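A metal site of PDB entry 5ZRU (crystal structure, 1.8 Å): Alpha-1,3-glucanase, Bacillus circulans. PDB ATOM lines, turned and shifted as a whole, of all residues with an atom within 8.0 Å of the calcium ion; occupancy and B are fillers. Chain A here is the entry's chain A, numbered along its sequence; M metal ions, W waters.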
ATOM      1  N   GLY A 193     -10.034   0.416 -12.333  1.00  0.00           N
ATOM      2  CA  GLY A 193      -8.826   0.875 -12.970  1.00  0.00           C
ATOM      3  C   GLY A 193      -7.781  -0.194 -13.219  1.00  0.00           C
ATOM      4  O   GLY A 193      -6.771   0.110 -13.861  1.00  0.00           O
ATOM      5  N   ALA A 194      -7.977  -1.408 -12.721  1.00  0.00           N
ATOM      6  CA  ALA A 194      -7.013  -2.467 -13.015  1.00  0.00           C
ATOM      7  C   ALA A 194      -7.010  -2.769 -14.507  1.00  0.00           C
ATOM      8  O   ALA A 194      -8.067  -2.764 -15.149  1.00  0.00           O
ATOM      9  CB  ALA A 194      -7.322  -3.732 -12.228  1.00  0.00           C
ATOM     10  N   VAL A 195      -5.831  -3.031 -15.054  1.00  0.00           N
ATOM     11  CA  VAL A 195      -5.669  -3.380 -16.453  1.00  0.00           C
ATOM     12  C   VAL A 195      -4.805  -4.632 -16.538  1.00  0.00           C
ATOM     13  O   VAL A 195      -3.707  -4.669 -15.970  1.00  0.00           O
ATOM     14  CB  VAL A 195      -5.036  -2.233 -17.279  1.00  0.00           C
ATOM     15  CG1 VAL A 195      -4.865  -2.652 -18.732  1.00  0.00           C
ATOM     16  CG2 VAL A 195      -5.898  -0.966 -17.195  1.00  0.00           C
ATOM     17  N   ALA A 196      -5.305  -5.651 -17.232  1.00  0.00           N
ATOM     18  CA  ALA A 196      -4.527  -6.868 -17.410  1.00  0.00           C
ATOM     19  C   ALA A 196      -3.391  -6.671 -18.418  1.00  0.00           C
ATOM     20  O   ALA A 196      -3.526  -5.907 -19.381  1.00  0.00           O
ATOM     21  CB  ALA A 196      -5.433  -8.010 -17.887  1.00  0.00           C
ATOM     22  N   ASN A 197      -2.268  -7.341 -18.171  1.00  0.00           N
ATOM     23  CA  ASN A 197      -1.232  -7.595 -19.174  1.00  0.00           C
ATOM     24  C   ASN A 197      -0.469  -6.351 -19.608  1.00  0.00           C
ATOM     25  O   ASN A 197       0.175  -6.360 -20.665  1.00  0.00           O
ATOM     26  CB  ASN A 197      -1.826  -8.289 -20.413  1.00  0.00           C
ATOM     27  CG  ASN A 197      -2.549  -9.589 -20.080  1.00  0.00           C
ATOM     28  OD1 ASN A 197      -2.214 -10.262 -19.108  1.00  0.00           O
ATOM     29  ND2 ASN A 197      -3.547  -9.934 -20.887  1.00  0.00           N
ATOM     30  N   ASP A 198      -0.488  -5.274 -18.833  1.00  0.00           N
ATOM     31  CA  ASP A 198       0.237  -4.063 -19.207  1.00  0.00           C
ATOM     32  C   ASP A 198       1.478  -3.832 -18.362  1.00  0.00           C
ATOM     33  O   ASP A 198       2.157  -2.818 -18.555  1.00  0.00           O
ATOM     34  CB  ASP A 198      -0.699  -2.843 -19.143  1.00  0.00           C
ATOM     35  CG  ASP A 198      -1.123  -2.481 -17.728  1.00  0.00           C
ATOM     36  OD1 ASP A 198      -0.826  -3.235 -16.769  1.00  0.00           O
ATOM     37  OD2 ASP A 198      -1.768  -1.416 -17.567  1.00  0.00           O
ATOM     38  N   GLY A 199       1.801  -4.736 -17.446  1.00  0.00           N
ATOM     39  CA  GLY A 199       2.937  -4.545 -16.580  1.00  0.00           C
ATOM     40  C   GLY A 199       2.802  -3.456 -15.555  1.00  0.00           C
ATOM     41  O   GLY A 199       3.736  -3.225 -14.786  1.00  0.00           O
ATOM     42  N   GLN A 200       1.659  -2.765 -15.508  1.00  0.00           N
ATOM     43  CA  GLN A 200       1.453  -1.676 -14.563  1.00  0.00           C
ATOM     44  C   GLN A 200       0.763  -2.178 -13.306  1.00  0.00           C
ATOM     45  O   GLN A 200      -0.021  -3.140 -13.340  1.00  0.00           O
ATOM     46  CB  GLN A 200       0.612  -0.558 -15.182  1.00  0.00           C
ATOM     47  CG  GLN A 200       1.018  -0.142 -16.579  1.00  0.00           C
ATOM     48  CD  GLN A 200       2.360   0.507 -16.588  1.00  0.00           C
ATOM     49  OE1 GLN A 200       2.519   1.657 -16.156  1.00  0.00           O
ATOM     50  NE2 GLN A 200       3.371  -0.219 -17.065  1.00  0.00           N
ATOM     51  N   ASP A 201       1.034  -1.506 -12.194  1.00  0.00           N
ATOM     52  CA  ASP A 201       0.559  -1.953 -10.898  1.00  0.00           C
ATOM     53  C   ASP A 201      -0.957  -1.800 -10.767  1.00  0.00           C
ATOM     54  O   ASP A 201      -1.517  -0.750 -11.086  1.00  0.00           O
ATOM     55  CB  ASP A 201       1.279  -1.187  -9.799  1.00  0.00           C
ATOM     56  CG  ASP A 201       1.153  -1.865  -8.444  1.00  0.00           C
ATOM     57  OD1 ASP A 201       0.033  -1.972  -7.921  1.00  0.00           O
ATOM     58  OD2 ASP A 201       2.184  -2.302  -7.908  1.00  0.00           O
ATOM     59  N   ASP A 202      -1.610  -2.848 -10.236  1.00  0.00           N
ATOM     60  CA  ASP A 202      -3.053  -2.886 -10.106  1.00  0.00           C
ATOM     61  C   ASP A 202      -3.533  -2.849  -8.660  1.00  0.00           C
ATOM     62  O   ASP A 202      -4.751  -2.909  -8.422  1.00  0.00           O
ATOM     63  CB  ASP A 202      -3.596  -4.148 -10.791  1.00  0.00           C
ATOM     64  CG  ASP A 202      -3.209  -4.221 -12.250  1.00  0.00           C
ATOM     65  OD1 ASP A 202      -3.678  -3.357 -13.029  1.00  0.00           O
ATOM     66  OD2 ASP A 202      -2.405  -5.109 -12.622  1.00  0.00           O
ATOM     67  N   LEU A 203      -2.627  -2.759  -7.685  1.00  0.00           N
ATOM     68  CA  LEU A 203      -3.030  -2.967  -6.289  1.00  0.00           C
ATOM     69  C   LEU A 203      -3.961  -1.872  -5.790  1.00  0.00           C
ATOM     70  O   LEU A 203      -4.846  -2.148  -4.966  1.00  0.00           O
ATOM     71  CB  LEU A 203      -1.798  -3.083  -5.395  1.00  0.00           C
ATOM     72  CG  LEU A 203      -2.059  -3.315  -3.901  1.00  0.00           C
ATOM     73  CD1 LEU A 203      -2.933  -4.547  -3.657  1.00  0.00           C
ATOM     74  CD2 LEU A 203      -0.748  -3.451  -3.134  1.00  0.00           C
ATOM     75  N   PHE A 206      -7.285  -3.028  -6.943  1.00  0.00           N
ATOM     76  CA  PHE A 206      -7.729  -4.179  -6.150  1.00  0.00           C
ATOM     77  C   PHE A 206      -8.253  -3.739  -4.791  1.00  0.00           C
ATOM     78  O   PHE A 206      -9.298  -4.228  -4.334  1.00  0.00           O
ATOM     79  CB  PHE A 206      -6.568  -5.166  -5.954  1.00  0.00           C
ATOM     80  CG  PHE A 206      -6.404  -6.144  -7.073  1.00  0.00           C
ATOM     81  CD1 PHE A 206      -6.403  -5.732  -8.405  1.00  0.00           C
ATOM     82  CD2 PHE A 206      -6.188  -7.487  -6.800  1.00  0.00           C
ATOM     83  CE1 PHE A 206      -6.225  -6.655  -9.417  1.00  0.00           C
ATOM     84  CE2 PHE A 206      -5.994  -8.413  -7.823  1.00  0.00           C
ATOM     85  CZ  PHE A 206      -6.016  -7.997  -9.138  1.00  0.00           C
ATOM     86  N   THR A 226      -3.061 -11.067 -16.559  1.00  0.00           N
ATOM     87  CA  THR A 226      -2.065 -10.929 -15.508  1.00  0.00           C
ATOM     88  C   THR A 226      -2.182  -9.551 -14.865  1.00  0.00           C
ATOM     89  O   THR A 226      -2.133  -8.526 -15.563  1.00  0.00           O
ATOM     90  CB  THR A 226      -0.649 -11.121 -16.058  1.00  0.00           C
ATOM     91  OG1 THR A 226      -0.511 -12.458 -16.564  1.00  0.00           O
ATOM     92  CG2 THR A 226       0.391 -10.893 -14.955  1.00  0.00           C
ATOM     93  N   PHE A 227      -2.332  -9.538 -13.544  1.00  0.00           N
ATOM     94  CA  PHE A 227      -2.390  -8.319 -12.760  1.00  0.00           C
ATOM     95  C   PHE A 227      -1.190  -8.270 -11.834  1.00  0.00           C
ATOM     96  O   PHE A 227      -0.760  -9.294 -11.306  1.00  0.00           O
ATOM     97  CB  PHE A 227      -3.699  -8.265 -11.972  1.00  0.00           C
ATOM     98  CG  PHE A 227      -4.895  -8.261 -12.855  1.00  0.00           C
ATOM     99  CD1 PHE A 227      -5.438  -7.070 -13.293  1.00  0.00           C
ATOM    100  CD2 PHE A 227      -5.443  -9.465 -13.306  1.00  0.00           C
ATOM    101  CE1 PHE A 227      -6.550  -7.063 -14.131  1.00  0.00           C
ATOM    102  CE2 PHE A 227      -6.537  -9.468 -14.149  1.00  0.00           C
ATOM    103  CZ  PHE A 227      -7.090  -8.266 -14.553  1.00  0.00           C
ATOM    104  N   HIS A 228      -0.631  -7.063 -11.661  1.00  0.00           N
ATOM    105  CA  HIS A 228       0.626  -6.886 -10.952  1.00  0.00           C
ATOM    106  C   HIS A 228       0.373  -6.135  -9.651  1.00  0.00           C
ATOM    107  O   HIS A 228      -0.207  -5.041  -9.666  1.00  0.00           O
ATOM    108  CB  HIS A 228       1.646  -6.140 -11.824  1.00  0.00           C
ATOM    109  CG  HIS A 228       2.114  -6.947 -13.004  1.00  0.00           C
ATOM    110  ND1 HIS A 228       1.459  -6.927 -14.215  1.00  0.00           N
ATOM    111  CD2 HIS A 228       3.156  -7.800 -13.144  1.00  0.00           C
ATOM    112  CE1 HIS A 228       2.096  -7.725 -15.063  1.00  0.00           C
ATOM    113  NE2 HIS A 228       3.121  -8.277 -14.434  1.00  0.00           N
ATOM    114  N   LEU A 229       0.815  -6.716  -8.542  1.00  0.00           N
ATOM    115  CA  LEU A 229       0.587  -6.146  -7.224  1.00  0.00           C
ATOM    116  C   LEU A 229       1.939  -5.887  -6.562  1.00  0.00           C
ATOM    117  O   LEU A 229       2.649  -6.830  -6.223  1.00  0.00           O
ATOM    118  CB  LEU A 229      -0.280  -7.075  -6.367  1.00  0.00           C
ATOM    119  CG  LEU A 229      -1.619  -7.519  -6.961  1.00  0.00           C
ATOM    120  CD1 LEU A 229      -2.410  -8.290  -5.907  1.00  0.00           C
ATOM    121  CD2 LEU A 229      -2.448  -6.335  -7.428  1.00  0.00           C
HETATM  122 CA    CA M   1      -1.925  -3.829 -14.690  1.00  0.00          CA
HETATM  123  O   HOH W   1      -2.586  -1.473 -15.028  1.00  0.00           O
HETATM  124  O   HOH W   2      -0.782  -6.018 -15.284  1.00  0.00           O
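N of Asp 202 is in hydrogen-bond range of O of His 228 (2.7 Å).
Within 4 Å of the calcium ion: Val 195, Asp 198, Gln 200 and Asp 202.
The nearest printed residue that does not touch the calcium ion is Asp 201 (4.5 Å).
The calcium ion is bound by O of Val 195.
The calcium ion is bound by OD1 of Asp 198 (2.4 Å).
The calcium ion is bound by O of Gln 200, at 2.4 Å.
The side-chain carboxylate (OD1) of Asp 202 binds the calcium ion.
Water W1 binds the calcium ion (2.5 Å).
The calcium ion is bound by OD2 of Asp 202 (2.5 Å).
The calcium ion is bound by water W2, at 2.5 Å.
Water W2 bridges a ring nitrogen (ND1) of His 228 (2.6 Å) and the backbone carbonyl oxygen of Thr 226 (2.9 Å).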
